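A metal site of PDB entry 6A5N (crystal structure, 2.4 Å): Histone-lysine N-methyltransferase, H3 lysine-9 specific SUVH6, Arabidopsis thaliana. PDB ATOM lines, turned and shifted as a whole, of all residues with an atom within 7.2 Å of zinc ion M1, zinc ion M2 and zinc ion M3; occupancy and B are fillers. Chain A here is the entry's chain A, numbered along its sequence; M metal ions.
Zinc ion M1 is bound by SG of Cys 306 (2.2 Å), SG of Cys 336 (2.4 Å), SG of Cys 290 (2.4 Å) and SG of Cys 332 (2.6 Å).
Zinc ion M3 is bound by SG of Cys 304, SG of Cys 296, SG of Cys 292 and SG of Cys 290. Zinc ion M3 has four donor atoms within binding distance.
Within 4 Å of zinc ion M3: Cys 290, Cys 292, Cys 296 and Cys 304.
Of the 29 residues printed, 4 come within 4 Å of zinc ion M1. Along chain A the residues within 4 Å of zinc ion M1 span positions 290 to 336. The nearest printed residue that does not touch zinc ion M1 is Ser 289 (4.4 Å).
SG of Cys 332 binds zinc ion M2 (2.1 Å). Zinc ion M2 is bound by SG of Cys 296 (2.2 Å). SG of Cys 338 is bound to zinc ion M2, at 2.4 Å. Zinc ion M2 is bound by SG of Cys 342, at 2.7 Å.
The backbone NH of Cys 332 sits at hydrogen-bond distance from the backbone carbonyl oxygen of Leu 344 (3.1 Å). The backbone NH of Lys 337 is in hydrogen-bond range of the backbone carbonyl oxygen of Cys 290 (3.5 Å). The side-chain sulfur of Cys 304 lies close to the backbone NH of Val 307 (3.3 Å). The side-chain sulfur of Cys 336 lies close to the backbone NH of Gly 333. N of Cys 306 lies close to SG of Cys 304, 3.2 Å away. O of Cys 332 sits at hydrogen-bond distance from NH2 of Arg 345. O of Cys 338 lies within hydrogen-bond range of NH1 of Arg 345 (3.2 Å). The backbone carbonyl oxygen (O) of Cys 292 sits at hydrogen-bond distance from the backbone NH (N) of Cys 338 (3.4 Å).
Within 4 Å of zinc ion M2: Cys 290, Cys 296, Cys 332, Cys 338 and Cys 342.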
ATOM      1  N   LYS A 288      18.273  -8.305  22.803  1.00  0.00           N
ATOM      2  CA  LYS A 288      18.610  -9.412  21.917  1.00  0.00           C
ATOM      3  C   LYS A 288      17.541  -9.487  20.805  1.00  0.00           C
ATOM      4  O   LYS A 288      16.366  -9.239  21.065  1.00  0.00           O
ATOM      5  CB  LYS A 288      18.701 -10.727  22.701  1.00  0.00           C
ATOM      6  CG  LYS A 288      20.044 -11.478  22.557  1.00  0.00           C
ATOM      7  CD  LYS A 288      21.077 -10.994  23.578  1.00  0.00           C
ATOM      8  CE  LYS A 288      22.440 -11.666  23.402  1.00  0.00           C
ATOM      9  NZ  LYS A 288      22.927 -11.582  22.006  1.00  0.00           N
ATOM     10  N   SER A 289      17.971  -9.796  19.574  1.00  0.00           N
ATOM     11  CA  SER A 289      17.095  -9.817  18.390  1.00  0.00           C
ATOM     12  C   SER A 289      17.143 -11.173  17.680  1.00  0.00           C
ATOM     13  O   SER A 289      18.035 -11.976  17.957  1.00  0.00           O
ATOM     14  CB  SER A 289      17.517  -8.707  17.410  1.00  0.00           C
ATOM     15  OG  SER A 289      17.592  -7.451  18.065  1.00  0.00           O
ATOM     16  N   CYS A 290      16.189 -11.438  16.777  1.00  0.00           N
ATOM     17  CA  CYS A 290      16.190 -12.687  16.002  1.00  0.00           C
ATOM     18  C   CYS A 290      16.842 -12.490  14.646  1.00  0.00           C
ATOM     19  O   CYS A 290      16.997 -11.362  14.183  1.00  0.00           O
ATOM     20  CB  CYS A 290      14.759 -13.243  15.842  1.00  0.00           C
ATOM     21  SG  CYS A 290      13.662 -12.348  14.682  1.00  0.00           S
ATOM     22  N   CYS A 291      17.191 -13.597  13.983  1.00  0.00           N
ATOM     23  CA  CYS A 291      17.891 -13.549  12.710  1.00  0.00           C
ATOM     24  C   CYS A 291      17.047 -14.066  11.540  1.00  0.00           C
ATOM     25  O   CYS A 291      17.590 -14.342  10.470  1.00  0.00           O
ATOM     26  CB  CYS A 291      19.194 -14.355  12.808  1.00  0.00           C
ATOM     27  SG  CYS A 291      20.247 -13.886  14.174  1.00  0.00           S
ATOM     28  N   CYS A 292      15.741 -14.185  11.737  1.00  0.00           N
ATOM     29  CA  CYS A 292      14.878 -14.818  10.750  1.00  0.00           C
ATOM     30  C   CYS A 292      14.764 -14.034   9.424  1.00  0.00           C
ATOM     31  O   CYS A 292      14.576 -12.809   9.428  1.00  0.00           O
ATOM     32  CB  CYS A 292      13.493 -15.065  11.349  1.00  0.00           C
ATOM     33  SG  CYS A 292      13.439 -16.198  12.796  1.00  0.00           S
ATOM     34  N   THR A 293      14.897 -14.750   8.311  1.00  0.00           N
ATOM     35  CA  THR A 293      14.755 -14.194   6.957  1.00  0.00           C
ATOM     36  C   THR A 293      13.280 -13.907   6.683  1.00  0.00           C
ATOM     37  O   THR A 293      12.917 -12.819   6.227  1.00  0.00           O
ATOM     38  CB  THR A 293      15.260 -15.159   5.854  1.00  0.00           C
ATOM     39  OG1 THR A 293      14.395 -16.297   5.774  1.00  0.00           O
ATOM     40  CG2 THR A 293      16.688 -15.622   6.129  1.00  0.00           C
ATOM     41  N   THR A 294      12.459 -14.912   6.950  1.00  0.00           N
ATOM     42  CA  THR A 294      11.014 -14.852   6.758  1.00  0.00           C
ATOM     43  C   THR A 294      10.290 -14.385   8.037  1.00  0.00           C
ATOM     44  O   THR A 294      10.940 -13.910   8.973  1.00  0.00           O
ATOM     45  CB  THR A 294      10.465 -16.220   6.322  1.00  0.00           C
ATOM     46  OG1 THR A 294       9.039 -16.141   6.116  1.00  0.00           O
ATOM     47  CG2 THR A 294      10.770 -17.274   7.381  1.00  0.00           C
ATOM     48  N   ARG A 295       8.964 -14.506   8.064  1.00  0.00           N
ATOM     49  CA  ARG A 295       8.164 -14.148   9.241  1.00  0.00           C
ATOM     50  C   ARG A 295       8.383 -15.117  10.386  1.00  0.00           C
ATOM     51  O   ARG A 295       8.504 -16.328  10.183  1.00  0.00           O
ATOM     52  CB  ARG A 295       6.682 -14.089   8.893  1.00  0.00           C
ATOM     53  CG  ARG A 295       6.310 -12.962   7.957  1.00  0.00           C
ATOM     54  CD  ARG A 295       4.808 -12.917   7.747  1.00  0.00           C
ATOM     55  NE  ARG A 295       4.369 -14.093   7.008  1.00  0.00           N
ATOM     56  CZ  ARG A 295       3.415 -14.075   6.081  1.00  0.00           C
ATOM     57  NH1 ARG A 295       3.080 -15.196   5.455  1.00  0.00           N
ATOM     58  NH2 ARG A 295       2.806 -12.948   5.788  1.00  0.00           N
ATOM     59  N   CYS A 296       8.416 -14.592  11.614  1.00  0.00           N
ATOM     60  CA  CYS A 296       8.742 -15.420  12.764  1.00  0.00           C
ATOM     61  C   CYS A 296       7.546 -16.233  13.202  1.00  0.00           C
ATOM     62  O   CYS A 296       6.508 -15.693  13.623  1.00  0.00           O
ATOM     63  CB  CYS A 296       9.251 -14.558  13.910  1.00  0.00           C
ATOM     64  SG  CYS A 296      10.663 -13.564  13.442  1.00  0.00           S
ATOM     65  N   THR A 297       7.675 -17.548  13.073  1.00  0.00           N
ATOM     66  CA  THR A 297       6.606 -18.453  13.475  1.00  0.00           C
ATOM     67  C   THR A 297       7.222 -19.645  14.165  1.00  0.00           C
ATOM     68  O   THR A 297       8.413 -19.917  13.981  1.00  0.00           O
ATOM     69  CB  THR A 297       5.767 -18.939  12.275  1.00  0.00           C
ATOM     70  OG1 THR A 297       6.456 -20.020  11.637  1.00  0.00           O
ATOM     71  CG2 THR A 297       5.517 -17.823  11.289  1.00  0.00           C
ATOM     72  N   ARG A 302      13.953 -23.316  11.374  1.00  0.00           N
ATOM     73  CA  ARG A 302      14.850 -22.520  12.188  1.00  0.00           C
ATOM     74  C   ARG A 302      14.124 -21.887  13.354  1.00  0.00           C
ATOM     75  O   ARG A 302      13.032 -21.341  13.201  1.00  0.00           O
ATOM     76  CB  ARG A 302      15.544 -21.432  11.359  1.00  0.00           C
ATOM     77  CG  ARG A 302      16.483 -21.947  10.264  1.00  0.00           C
ATOM     78  CD  ARG A 302      16.972 -20.768   9.407  1.00  0.00           C
ATOM     79  NE  ARG A 302      16.911 -19.534  10.195  1.00  0.00           N
ATOM     80  CZ  ARG A 302      17.580 -18.423   9.898  1.00  0.00           C
ATOM     81  NH1 ARG A 302      18.348 -18.358   8.816  1.00  0.00           N
ATOM     82  NH2 ARG A 302      17.463 -17.364  10.689  1.00  0.00           N
ATOM     83  N   VAL A 303      14.740 -21.981  14.531  1.00  0.00           N
ATOM     84  CA  VAL A 303      14.208 -21.380  15.741  1.00  0.00           C
ATOM     85  C   VAL A 303      14.471 -19.878  15.759  1.00  0.00           C
ATOM     86  O   VAL A 303      15.492 -19.417  15.238  1.00  0.00           O
ATOM     87  CB  VAL A 303      14.818 -22.059  16.988  1.00  0.00           C
ATOM     88  CG1 VAL A 303      16.339 -22.066  16.918  1.00  0.00           C
ATOM     89  CG2 VAL A 303      14.347 -21.396  18.260  1.00  0.00           C
ATOM     90  N   CYS A 304      13.531 -19.132  16.334  1.00  0.00           N
ATOM     91  CA  CYS A 304      13.575 -17.673  16.442  1.00  0.00           C
ATOM     92  C   CYS A 304      13.774 -17.222  17.873  1.00  0.00           C
ATOM     93  O   CYS A 304      13.001 -17.600  18.752  1.00  0.00           O
ATOM     94  CB  CYS A 304      12.273 -17.062  15.910  1.00  0.00           C
ATOM     95  SG  CYS A 304      11.912 -15.401  16.578  1.00  0.00           S
ATOM     96  N   ALA A 305      14.785 -16.396  18.117  1.00  0.00           N
ATOM     97  CA  ALA A 305      15.100 -15.954  19.479  1.00  0.00           C
ATOM     98  C   ALA A 305      13.931 -15.261  20.197  1.00  0.00           C
ATOM     99  O   ALA A 305      13.805 -15.354  21.425  1.00  0.00           O
ATOM    100  CB  ALA A 305      16.300 -15.046  19.447  1.00  0.00           C
ATOM    101  N   CYS A 306      13.081 -14.546  19.441  1.00  0.00           N
ATOM    102  CA  CYS A 306      11.983 -13.816  20.052  1.00  0.00           C
ATOM    103  C   CYS A 306      10.814 -14.749  20.395  1.00  0.00           C
ATOM    104  O   CYS A 306      10.126 -14.557  21.412  1.00  0.00           O
ATOM    105  CB  CYS A 306      11.524 -12.682  19.137  1.00  0.00           C
ATOM    106  SG  CYS A 306      12.828 -11.505  18.623  1.00  0.00           S
ATOM    107  N   VAL A 307      10.608 -15.775  19.579  1.00  0.00           N
ATOM    108  CA  VAL A 307       9.715 -16.876  19.929  1.00  0.00           C
ATOM    109  C   VAL A 307      10.156 -17.540  21.236  1.00  0.00           C
ATOM    110  O   VAL A 307       9.390 -17.600  22.195  1.00  0.00           O
ATOM    111  CB  VAL A 307       9.678 -17.926  18.794  1.00  0.00           C
ATOM    112  CG1 VAL A 307       8.961 -19.189  19.247  1.00  0.00           C
ATOM    113  CG2 VAL A 307       8.978 -17.340  17.594  1.00  0.00           C
ATOM    114  N   LYS A 309      11.961 -16.323  23.478  1.00  0.00           N
ATOM    115  CA  LYS A 309      11.693 -15.339  24.526  1.00  0.00           C
ATOM    116  C   LYS A 309      10.223 -15.372  24.993  1.00  0.00           C
ATOM    117  O   LYS A 309       9.966 -15.219  26.185  1.00  0.00           O
ATOM    118  CB  LYS A 309      12.057 -13.930  24.051  1.00  0.00           C
ATOM    119  CG  LYS A 309      13.341 -13.405  24.645  1.00  0.00           C
ATOM    120  CD  LYS A 309      13.514 -11.916  24.416  1.00  0.00           C
ATOM    121  CE  LYS A 309      13.612 -11.580  22.941  1.00  0.00           C
ATOM    122  NZ  LYS A 309      14.007 -10.161  22.676  1.00  0.00           N
ATOM    123  N   GLU A 331       7.698  -8.503  21.368  1.00  0.00           N
ATOM    124  CA  GLU A 331       7.624  -8.332  19.924  1.00  0.00           C
ATOM    125  C   GLU A 331       9.030  -8.186  19.273  1.00  0.00           C
ATOM    126  O   GLU A 331       9.982  -7.782  19.948  1.00  0.00           O
ATOM    127  CB  GLU A 331       6.733  -7.136  19.588  1.00  0.00           C
ATOM    128  CG  GLU A 331       5.258  -7.519  19.480  1.00  0.00           C
ATOM    129  CD  GLU A 331       4.351  -6.350  19.136  1.00  0.00           C
ATOM    130  OE1 GLU A 331       4.635  -5.668  18.132  1.00  0.00           O
ATOM    131  OE2 GLU A 331       3.314  -6.172  19.822  1.00  0.00           O
ATOM    132  N   CYS A 332       9.132  -8.531  17.983  1.00  0.00           N
ATOM    133  CA  CYS A 332      10.392  -8.408  17.252  1.00  0.00           C
ATOM    134  C   CYS A 332      10.821  -6.940  17.198  1.00  0.00           C
ATOM    135  O   CYS A 332      10.011  -6.044  16.886  1.00  0.00           O
ATOM    136  CB  CYS A 332      10.248  -8.965  15.832  1.00  0.00           C
ATOM    137  SG  CYS A 332      10.419 -10.766  15.674  1.00  0.00           S
ATOM    138  N   GLY A 333      12.087  -6.685  17.512  1.00  0.00           N
ATOM    139  CA  GLY A 333      12.583  -5.318  17.560  1.00  0.00           C
ATOM    140  C   GLY A 333      13.077  -4.765  16.231  1.00  0.00           C
ATOM    141  O   GLY A 333      12.996  -5.433  15.202  1.00  0.00           O
ATOM    142  N   LEU A 335      16.077  -4.217  15.405  1.00  0.00           N
ATOM    143  CA  LEU A 335      17.308  -4.886  14.982  1.00  0.00           C
ATOM    144  C   LEU A 335      17.073  -6.393  14.741  1.00  0.00           C
ATOM    145  O   LEU A 335      18.019  -7.152  14.535  1.00  0.00           O
ATOM    146  CB  LEU A 335      18.416  -4.652  16.022  1.00  0.00           C
ATOM    147  CG  LEU A 335      18.891  -3.194  16.121  1.00  0.00           C
ATOM    148  CD1 LEU A 335      20.151  -3.038  16.966  1.00  0.00           C
ATOM    149  CD2 LEU A 335      19.106  -2.612  14.737  1.00  0.00           C
ATOM    150  N   CYS A 336      15.802  -6.800  14.759  1.00  0.00           N
ATOM    151  CA  CYS A 336      15.387  -8.086  14.203  1.00  0.00           C
ATOM    152  C   CYS A 336      15.383  -7.980  12.687  1.00  0.00           C
ATOM    153  O   CYS A 336      15.199  -6.887  12.158  1.00  0.00           O
ATOM    154  CB  CYS A 336      14.015  -8.473  14.739  1.00  0.00           C
ATOM    155  SG  CYS A 336      13.986  -8.817  16.506  1.00  0.00           S
ATOM    156  N   LYS A 337      15.587  -9.091  11.976  1.00  0.00           N
ATOM    157  CA  LYS A 337      15.796  -9.037  10.510  1.00  0.00           C
ATOM    158  C   LYS A 337      14.569  -9.449   9.683  1.00  0.00           C
ATOM    159  O   LYS A 337      14.619  -9.479   8.445  1.00  0.00           O
ATOM    160  CB  LYS A 337      16.993  -9.907  10.145  1.00  0.00           C
ATOM    161  CG  LYS A 337      18.350  -9.310  10.500  1.00  0.00           C
ATOM    162  CD  LYS A 337      18.581  -7.989   9.763  1.00  0.00           C
ATOM    163  CE  LYS A 337      19.591  -7.100  10.495  1.00  0.00           C
ATOM    164  NZ  LYS A 337      19.117  -5.693  10.701  1.00  0.00           N
ATOM    165  N   CYS A 338      13.491  -9.760  10.381  1.00  0.00           N
ATOM    166  CA  CYS A 338      12.206 -10.186   9.834  1.00  0.00           C
ATOM    167  C   CYS A 338      11.404  -9.067   9.174  1.00  0.00           C
ATOM    168  O   CYS A 338      11.474  -7.924   9.638  1.00  0.00           O
ATOM    169  CB  CYS A 338      11.373 -10.778  10.972  1.00  0.00           C
ATOM    170  SG  CYS A 338      11.342  -9.692  12.413  1.00  0.00           S
ATOM    171  N   PRO A 339      10.627  -9.384   8.124  1.00  0.00           N
ATOM    172  CA  PRO A 339       9.760  -8.409   7.460  1.00  0.00           C
ATOM    173  C   PRO A 339       8.723  -7.788   8.410  1.00  0.00           C
ATOM    174  O   PRO A 339       8.373  -8.443   9.389  1.00  0.00           O
ATOM    175  CB  PRO A 339       9.063  -9.235   6.370  1.00  0.00           C
ATOM    176  CG  PRO A 339       9.898 -10.437   6.174  1.00  0.00           C
ATOM    177  CD  PRO A 339      10.487 -10.736   7.530  1.00  0.00           C
ATOM    178  N   CYS A 342       5.828  -9.734   9.808  1.00  0.00           N
ATOM    179  CA  CYS A 342       6.040 -10.739  10.850  1.00  0.00           C
ATOM    180  C   CYS A 342       4.921 -10.717  11.897  1.00  0.00           C
ATOM    181  O   CYS A 342       4.485  -9.655  12.351  1.00  0.00           O
ATOM    182  CB  CYS A 342       7.397 -10.505  11.512  1.00  0.00           C
ATOM    183  SG  CYS A 342       7.634 -11.410  13.049  1.00  0.00           S
ATOM    184  N   TYR A 343       4.448 -11.900  12.266  1.00  0.00           N
ATOM    185  CA  TYR A 343       3.283 -12.018  13.130  1.00  0.00           C
ATOM    186  C   TYR A 343       3.633 -11.500  14.519  1.00  0.00           C
ATOM    187  O   TYR A 343       2.749 -11.140  15.304  1.00  0.00           O
ATOM    188  CB  TYR A 343       2.780 -13.468  13.172  1.00  0.00           C
ATOM    189  CG  TYR A 343       2.511 -14.075  11.809  1.00  0.00           C
ATOM    190  CD1 TYR A 343       1.511 -13.594  10.993  1.00  0.00           C
ATOM    191  CD2 TYR A 343       3.255 -15.147  11.354  1.00  0.00           C
ATOM    192  CE1 TYR A 343       1.265 -14.158   9.751  1.00  0.00           C
ATOM    193  CE2 TYR A 343       3.021 -15.713  10.120  1.00  0.00           C
ATOM    194  CZ  TYR A 343       2.027 -15.213   9.324  1.00  0.00           C
ATOM    195  OH  TYR A 343       1.793 -15.799   8.098  1.00  0.00           O
ATOM    196  N   LEU A 344       4.935 -11.469  14.812  1.00  0.00           N
ATOM    197  CA  LEU A 344       5.403 -10.969  16.100  1.00  0.00           C
ATOM    198  C   LEU A 344       5.618  -9.449  16.038  1.00  0.00           C
ATOM    199  O   LEU A 344       6.282  -8.863  16.905  1.00  0.00           O
ATOM    200  CB  LEU A 344       6.699 -11.696  16.524  1.00  0.00           C
ATOM    201  CG  LEU A 344       6.404 -13.094  17.065  1.00  0.00           C
ATOM    202  CD1 LEU A 344       7.626 -13.789  17.641  1.00  0.00           C
ATOM    203  CD2 LEU A 344       5.318 -13.035  18.106  1.00  0.00           C
ATOM    204  N   ARG A 345       5.028  -8.821  15.021  1.00  0.00           N
ATOM    205  CA  ARG A 345       4.860  -7.375  14.982  1.00  0.00           C
ATOM    206  C   ARG A 345       3.391  -7.006  14.918  1.00  0.00           C
ATOM    207  O   ARG A 345       2.759  -7.186  13.862  1.00  0.00           O
ATOM    208  CB  ARG A 345       5.583  -6.758  13.769  1.00  0.00           C
ATOM    209  CG  ARG A 345       6.990  -7.271  13.541  1.00  0.00           C
ATOM    210  CD  ARG A 345       7.800  -6.257  12.753  1.00  0.00           C
ATOM    211  NE  ARG A 345       9.139  -6.740  12.450  1.00  0.00           N
ATOM    212  CZ  ARG A 345      10.263  -6.205  12.928  1.00  0.00           C
ATOM    213  NH1 ARG A 345      11.436  -6.701  12.581  1.00  0.00           N
ATOM    214  NH2 ARG A 345      10.204  -5.174  13.754  1.00  0.00           N
HETATM  215 ZN    ZN M   1      12.897 -10.962  16.520  1.00  0.00          ZN
HETATM  216 ZN    ZN M   2      10.209 -11.436  13.676  1.00  0.00          ZN
HETATM  217 ZN    ZN M   3      12.576 -14.667  14.511  1.00  0.00          ZN
